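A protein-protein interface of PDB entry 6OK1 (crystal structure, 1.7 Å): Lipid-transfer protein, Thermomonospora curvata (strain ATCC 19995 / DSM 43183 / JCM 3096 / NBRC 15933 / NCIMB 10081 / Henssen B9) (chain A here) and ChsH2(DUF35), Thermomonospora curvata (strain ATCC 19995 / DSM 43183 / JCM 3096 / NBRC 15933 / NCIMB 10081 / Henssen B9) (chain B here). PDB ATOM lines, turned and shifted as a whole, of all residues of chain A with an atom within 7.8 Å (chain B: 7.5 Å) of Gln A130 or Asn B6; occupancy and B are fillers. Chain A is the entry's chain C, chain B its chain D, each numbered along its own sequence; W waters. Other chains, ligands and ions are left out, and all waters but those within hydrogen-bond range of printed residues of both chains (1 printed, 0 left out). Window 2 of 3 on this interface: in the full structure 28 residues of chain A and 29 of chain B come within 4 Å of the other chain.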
ATOM      1  N   ASP A 129      26.410  15.804  29.629  1.00  0.00           N
ATOM      2  CA  ASP A 129      25.508  14.674  29.438  1.00  0.00           C
ATOM      3  C   ASP A 129      24.696  14.854  28.139  1.00  0.00           C
ATOM      4  O   ASP A 129      25.053  15.648  27.268  1.00  0.00           O
ATOM      5  CB  ASP A 129      24.591  14.508  30.669  1.00  0.00           C
ATOM      6  CG  ASP A 129      23.691  15.721  30.926  1.00  0.00           C
ATOM      7  OD1 ASP A 129      23.334  16.430  29.981  1.00  0.00           O
ATOM      8  OD2 ASP A 129      23.344  15.974  32.093  1.00  0.00           O
ATOM      9  N   GLN A 130      23.619  14.094  27.990  1.00  0.00           N
ATOM     10  CA  GLN A 130      22.812  14.144  26.779  1.00  0.00           C
ATOM     11  C   GLN A 130      21.502  14.889  26.973  1.00  0.00           C
ATOM     12  O   GLN A 130      20.600  14.763  26.144  1.00  0.00           O
ATOM     13  CB  GLN A 130      22.539  12.729  26.267  1.00  0.00           C
ATOM     14  CG  GLN A 130      23.815  11.968  25.945  1.00  0.00           C
ATOM     15  CD  GLN A 130      23.715  11.126  24.690  1.00  0.00           C
ATOM     16  OE1 GLN A 130      22.656  11.033  24.056  1.00  0.00           O
ATOM     17  NE2 GLN A 130      24.833  10.510  24.315  1.00  0.00           N
ATOM     18  N   GLY A 131      21.385  15.680  28.036  1.00  0.00           N
ATOM     19  CA  GLY A 131      20.183  16.441  28.274  1.00  0.00           C
ATOM     20  C   GLY A 131      20.119  17.727  27.441  1.00  0.00           C
ATOM     21  O   GLY A 131      21.101  18.121  26.803  1.00  0.00           O
ATOM     22  N   ALA A 132      18.977  18.410  27.545  1.00  0.00           N
ATOM     23  CA  ALA A 132      18.735  19.613  26.748  1.00  0.00           C
ATOM     24  C   ALA A 132      19.663  20.758  27.142  1.00  0.00           C
ATOM     25  O   ALA A 132      20.057  21.568  26.289  1.00  0.00           O
ATOM     26  CB  ALA A 132      17.269  20.057  26.886  1.00  0.00           C
ATOM     27  N   ASP A 133      19.960  20.903  28.437  1.00  0.00           N
ATOM     28  CA  ASP A 133      20.841  21.993  28.871  1.00  0.00           C
ATOM     29  C   ASP A 133      22.235  21.839  28.255  1.00  0.00           C
ATOM     30  O   ASP A 133      22.823  22.805  27.763  1.00  0.00           O
ATOM     31  CB  ASP A 133      20.955  22.024  30.406  1.00  0.00           C
ATOM     32  CG  ASP A 133      19.664  22.390  31.095  1.00  0.00           C
ATOM     33  OD1 ASP A 133      19.551  22.132  32.313  1.00  0.00           O
ATOM     34  OD2 ASP A 133      18.758  22.932  30.446  1.00  0.00           O
ATOM     35  N   SER A 134      22.786  20.627  28.301  1.00  0.00           N
ATOM     36  CA  SER A 134      24.093  20.379  27.692  1.00  0.00           C
ATOM     37  C   SER A 134      24.038  20.567  26.191  1.00  0.00           C
ATOM     38  O   SER A 134      24.945  21.165  25.588  1.00  0.00           O
ATOM     39  CB  SER A 134      24.576  18.964  28.002  1.00  0.00           C
ATOM     40  OG  SER A 134      24.899  18.851  29.357  1.00  0.00           O
ATOM     41  N   ALA A 135      22.980  20.055  25.564  1.00  0.00           N
ATOM     42  CA  ALA A 135      22.873  20.115  24.117  1.00  0.00           C
ATOM     43  C   ALA A 135      22.780  21.547  23.597  1.00  0.00           C
ATOM     44  O   ALA A 135      23.114  21.797  22.434  1.00  0.00           O
ATOM     45  CB  ALA A 135      21.662  19.310  23.650  1.00  0.00           C
ATOM     46  N   ALA A 136      22.310  22.493  24.415  1.00  0.00           N
ATOM     47  CA  ALA A 136      22.187  23.874  23.937  1.00  0.00           C
ATOM     48  C   ALA A 136      23.545  24.438  23.523  1.00  0.00           C
ATOM     49  O   ALA A 136      23.616  25.354  22.701  1.00  0.00           O
ATOM     50  CB  ALA A 136      21.551  24.753  25.024  1.00  0.00           C
ATOM     51  N   ALA A 138      25.698  23.102  21.754  1.00  0.00           N
ATOM     52  CA  ALA A 138      26.089  22.686  20.404  1.00  0.00           C
ATOM     53  C   ALA A 138      26.024  23.850  19.421  1.00  0.00           C
ATOM     54  O   ALA A 138      26.718  23.830  18.396  1.00  0.00           O
ATOM     55  CB  ALA A 138      25.178  21.567  19.904  1.00  0.00           C
ATOM     56  N   ARG B   2      34.268  18.117  19.274  1.00  0.00           N
ATOM     57  CA  ARG B   2      32.992  17.424  19.117  1.00  0.00           C
ATOM     58  C   ARG B   2      31.905  18.138  19.954  1.00  0.00           C
ATOM     59  O   ARG B   2      32.045  18.263  21.171  1.00  0.00           O
ATOM     60  CB  ARG B   2      33.136  15.948  19.516  1.00  0.00           C
ATOM     61  CG  ARG B   2      31.903  15.072  19.246  1.00  0.00           C
ATOM     62  CD  ARG B   2      31.107  14.837  20.514  1.00  0.00           C
ATOM     63  NE  ARG B   2      30.192  13.696  20.411  1.00  0.00           N
ATOM     64  CZ  ARG B   2      30.337  12.530  21.043  1.00  0.00           C
ATOM     65  NH1 ARG B   2      31.363  12.318  21.857  1.00  0.00           N
ATOM     66  NH2 ARG B   2      29.437  11.566  20.867  1.00  0.00           N
ATOM     67  N   PRO B   3      30.840  18.623  19.309  1.00  0.00           N
ATOM     68  CA  PRO B   3      29.826  19.400  20.037  1.00  0.00           C
ATOM     69  C   PRO B   3      28.976  18.533  20.963  1.00  0.00           C
ATOM     70  O   PRO B   3      29.068  17.307  20.989  1.00  0.00           O
ATOM     71  CB  PRO B   3      28.977  20.012  18.915  1.00  0.00           C
ATOM     72  CG  PRO B   3      29.782  19.833  17.660  1.00  0.00           C
ATOM     73  CD  PRO B   3      30.551  18.595  17.863  1.00  0.00           C
ATOM     74  N   ALA B   4      28.110  19.216  21.720  1.00  0.00           N
ATOM     75  CA  ALA B   4      27.178  18.603  22.676  1.00  0.00           C
ATOM     76  C   ALA B   4      25.975  18.034  21.921  1.00  0.00           C
ATOM     77  O   ALA B   4      24.897  18.637  21.814  1.00  0.00           O
ATOM     78  CB  ALA B   4      26.752  19.634  23.699  1.00  0.00           C
ATOM     79  N   ILE B   5      26.178  16.844  21.387  1.00  0.00           N
ATOM     80  CA  ILE B   5      25.242  16.226  20.464  1.00  0.00           C
ATOM     81  C   ILE B   5      24.393  15.229  21.232  1.00  0.00           C
ATOM     82  O   ILE B   5      24.912  14.455  22.050  1.00  0.00           O
ATOM     83  CB  ILE B   5      25.995  15.549  19.305  1.00  0.00           C
ATOM     84  CG1 ILE B   5      26.712  16.625  18.477  1.00  0.00           C
ATOM     85  CG2 ILE B   5      25.033  14.737  18.432  1.00  0.00           C
ATOM     86  CD1 ILE B   5      27.457  16.110  17.263  1.00  0.00           C
ATOM     87  N   ASN B   6      23.085  15.264  20.995  1.00  0.00           N
ATOM     88  CA  ASN B   6      22.197  14.261  21.550  1.00  0.00           C
ATOM     89  C   ASN B   6      21.180  13.912  20.472  1.00  0.00           C
ATOM     90  O   ASN B   6      21.301  14.332  19.321  1.00  0.00           O
ATOM     91  CB  ASN B   6      21.567  14.739  22.870  1.00  0.00           C
ATOM     92  CG  ASN B   6      20.471  15.776  22.677  1.00  0.00           C
ATOM     93  OD1 ASN B   6      20.166  16.207  21.544  1.00  0.00           O
ATOM     94  ND2 ASN B   6      19.864  16.194  23.797  1.00  0.00           N
ATOM     95  N   ARG B   7      20.163  13.144  20.838  1.00  0.00           N
ATOM     96  CA  ARG B   7      19.244  12.642  19.819  1.00  0.00           C
ATOM     97  C   ARG B   7      18.447  13.733  19.122  1.00  0.00           C
ATOM     98  O   ARG B   7      17.926  13.491  18.026  1.00  0.00           O
ATOM     99  CB  ARG B   7      18.272  11.646  20.447  1.00  0.00           C
ATOM    100  CG  ARG B   7      18.994  10.402  20.962  1.00  0.00           C
ATOM    101  CD  ARG B   7      18.108   9.171  21.057  1.00  0.00           C
ATOM    102  NE  ARG B   7      17.844   8.794  22.439  1.00  0.00           N
ATOM    103  CZ  ARG B   7      17.670   7.548  22.874  1.00  0.00           C
ATOM    104  NH1 ARG B   7      17.749   6.506  22.048  1.00  0.00           N
ATOM    105  NH2 ARG B   7      17.419   7.345  24.158  1.00  0.00           N
ATOM    106  N   ASP B   8      18.320  14.908  19.733  1.00  0.00           N
ATOM    107  CA  ASP B   8      17.454  15.942  19.211  1.00  0.00           C
ATOM    108  C   ASP B   8      18.194  16.925  18.308  1.00  0.00           C
ATOM    109  O   ASP B   8      17.538  17.719  17.636  1.00  0.00           O
ATOM    110  CB  ASP B   8      16.761  16.699  20.357  1.00  0.00           C
ATOM    111  CG  ASP B   8      15.785  15.829  21.137  1.00  0.00           C
ATOM    112  OD1 ASP B   8      15.257  14.867  20.538  1.00  0.00           O
ATOM    113  OD2 ASP B   8      15.570  16.090  22.351  1.00  0.00           O
ATOM    114  N   ASN B   9      19.538  16.909  18.278  1.00  0.00           N
ATOM    115  CA  ASN B   9      20.274  17.771  17.342  1.00  0.00           C
ATOM    116  C   ASN B   9      21.276  17.022  16.461  1.00  0.00           C
ATOM    117  O   ASN B   9      21.952  17.657  15.639  1.00  0.00           O
ATOM    118  CB  ASN B   9      21.005  18.898  18.092  1.00  0.00           C
ATOM    119  CG  ASN B   9      22.079  18.393  19.049  1.00  0.00           C
ATOM    120  OD1 ASN B   9      22.527  17.259  18.948  1.00  0.00           O
ATOM    121  ND2 ASN B   9      22.526  19.263  19.957  1.00  0.00           N
ATOM    122  N   ALA B  10      21.391  15.704  16.604  1.00  0.00           N
ATOM    123  CA  ALA B  10      22.359  14.945  15.809  1.00  0.00           C
ATOM    124  C   ALA B  10      22.113  15.104  14.312  1.00  0.00           C
ATOM    125  O   ALA B  10      23.066  15.182  13.522  1.00  0.00           O
ATOM    126  CB  ALA B  10      22.313  13.467  16.214  1.00  0.00           C
ATOM    127  N   PHE B  11      20.842  15.155  13.900  1.00  0.00           N
ATOM    128  CA  PHE B  11      20.526  15.273  12.471  1.00  0.00           C
ATOM    129  C   PHE B  11      21.235  16.469  11.848  1.00  0.00           C
ATOM    130  O   PHE B  11      21.692  16.416  10.697  1.00  0.00           O
ATOM    131  CB  PHE B  11      19.008  15.410  12.292  1.00  0.00           C
ATOM    132  CG  PHE B  11      18.488  16.772  12.634  1.00  0.00           C
ATOM    133  CD1 PHE B  11      18.212  17.121  13.957  1.00  0.00           C
ATOM    134  CD2 PHE B  11      18.298  17.721  11.650  1.00  0.00           C
ATOM    135  CE1 PHE B  11      17.751  18.390  14.280  1.00  0.00           C
ATOM    136  CE2 PHE B  11      17.831  19.004  11.971  1.00  0.00           C
ATOM    137  CZ  PHE B  11      17.560  19.335  13.281  1.00  0.00           C
ATOM    138  N   TRP B  12      21.314  17.578  12.584  1.00  0.00           N
ATOM    139  CA  TRP B  12      21.866  18.796  11.998  1.00  0.00           C
ATOM    140  C   TRP B  12      23.357  18.642  11.708  1.00  0.00           C
ATOM    141  O   TRP B  12      23.847  19.090  10.661  1.00  0.00           O
ATOM    142  CB  TRP B  12      21.619  19.966  12.933  1.00  0.00           C
ATOM    143  CG  TRP B  12      21.901  21.289  12.318  1.00  0.00           C
ATOM    144  CD1 TRP B  12      21.011  22.089  11.664  1.00  0.00           C
ATOM    145  CD2 TRP B  12      23.150  21.995  12.323  1.00  0.00           C
ATOM    146  NE1 TRP B  12      21.626  23.245  11.266  1.00  0.00           N
ATOM    147  CE2 TRP B  12      22.939  23.212  11.652  1.00  0.00           C
ATOM    148  CE3 TRP B  12      24.424  21.718  12.838  1.00  0.00           C
ATOM    149  CZ2 TRP B  12      23.947  24.152  11.483  1.00  0.00           C
ATOM    150  CZ3 TRP B  12      25.423  22.652  12.672  1.00  0.00           C
ATOM    151  CH2 TRP B  12      25.184  23.852  11.992  1.00  0.00           C
ATOM    152  N   PHE B  13      24.095  18.027  12.631  1.00  0.00           N
ATOM    153  CA  PHE B  13      25.530  17.818  12.449  1.00  0.00           C
ATOM    154  C   PHE B  13      25.824  16.699  11.458  1.00  0.00           C
ATOM    155  O   PHE B  13      26.818  16.777  10.724  1.00  0.00           O
ATOM    156  CB  PHE B  13      26.182  17.562  13.819  1.00  0.00           C
ATOM    157  CG  PHE B  13      26.167  18.781  14.686  1.00  0.00           C
ATOM    158  CD1 PHE B  13      25.101  19.043  15.534  1.00  0.00           C
ATOM    159  CD2 PHE B  13      27.167  19.733  14.573  1.00  0.00           C
ATOM    160  CE1 PHE B  13      25.066  20.203  16.293  1.00  0.00           C
ATOM    161  CE2 PHE B  13      27.130  20.904  15.334  1.00  0.00           C
ATOM    162  CZ  PHE B  13      26.066  21.136  16.192  1.00  0.00           C
ATOM    163  N   GLU B  14      24.965  15.679  11.393  1.00  0.00           N
ATOM    164  CA  GLU B  14      25.076  14.676  10.335  1.00  0.00           C
ATOM    165  C   GLU B  14      24.915  15.308   8.953  1.00  0.00           C
ATOM    166  O   GLU B  14      25.681  15.002   8.030  1.00  0.00           O
ATOM    167  CB  GLU B  14      24.034  13.573  10.529  1.00  0.00           C
ATOM    168  CG  GLU B  14      24.268  12.674  11.751  1.00  0.00           C
ATOM    169  CD  GLU B  14      23.050  11.831  12.104  1.00  0.00           C
ATOM    170  OE1 GLU B  14      23.124  11.067  13.090  1.00  0.00           O
ATOM    171  OE2 GLU B  14      22.016  11.940  11.405  1.00  0.00           O
HETATM  172  O   HOH W   1      20.446  21.303  20.861  1.00  0.00           O
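Water W1 bridges the side-chain amide nitrogen (ND2) of Asn B9 and the backbone carbonyl oxygen (O) of Ala A135.
O of Gln A130 lies within hydrogen-bond range of ND2 of Asn B6, at 2.8 Å.
Gln A130 touches just one residue of chain B: Asn B6 (2.8 Å).
Ala A132 touches none of the printed residues of chain B.
Of the printed residues of chain B, Ala A135 touches Ala B4, Asn B6 and Asn B9.
Of the printed residues of chain B, Ala A138 touches Ala B4 (3.5 Å), Asn B9 (3.5 Å) and Phe B13 (3.5 Å).
Asn B6 touches just these residues of chain A: Gln A130, Gly A131 and Ala A135.
The nearest residue of chain A that does not touch Asn B6 is Ala A132 (4.4 Å).
Among the printed residues, merely in contact across the chains: Ser A134 with Ala B4 (3.0 Å), Ala A135 with Ala B4 (3.4 Å), Ala A138 with Ala B4 (3.5 Å), Ala A138 with Asn B9 (3.5 Å), Ala A138 with Phe B13 (3.5 Å), Ala A135 with Asn B9 (3.6 Å), Ala A135 with Asn B6 (3.6 Å) and Gly A131 with Asn B6 (3.8 Å).
The side-chain hydroxyl of Ser A134 is in hydrogen-bond range of the side-chain carboxylate of Asp A129, at 2.9 Å.
N of Asn B6 lies within hydrogen-bond range of OD1 of Asn B9, at 2.9 Å.
The side-chain carboxylate of Asp A129 lies within hydrogen-bond range of the backbone NH of Gly A131.
The side-chain amide oxygen (OD1) of Asn B6 is in hydrogen-bond range of the backbone NH (N) of Asp B8 (2.9 Å).
The backbone carbonyl oxygen (O) of Ala B4 is in hydrogen-bond range of the side-chain amide nitrogen (ND2) of Asn B9.
Of the 9 printed residues of chain A, 5 touch a printed residue of chain B.
Hydrophobic or aromatic side chains of chain A within 4 Å of the printed part of chain B: Ala A135 and Ala A138.
Of the 13 printed residues of chain B, 4 touch a printed residue of chain A.
Printed residues of chain B that touch a printed residue of chain A: Ala B4, Asn B6, Asn B9 and Phe B13.
Among the printed residues, 9 pairs touch across the chains.
Among the printed residues, no Asp or Glu carboxylate lies within 4 Å of a Lys or Arg side-chain nitrogen of the other chain.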
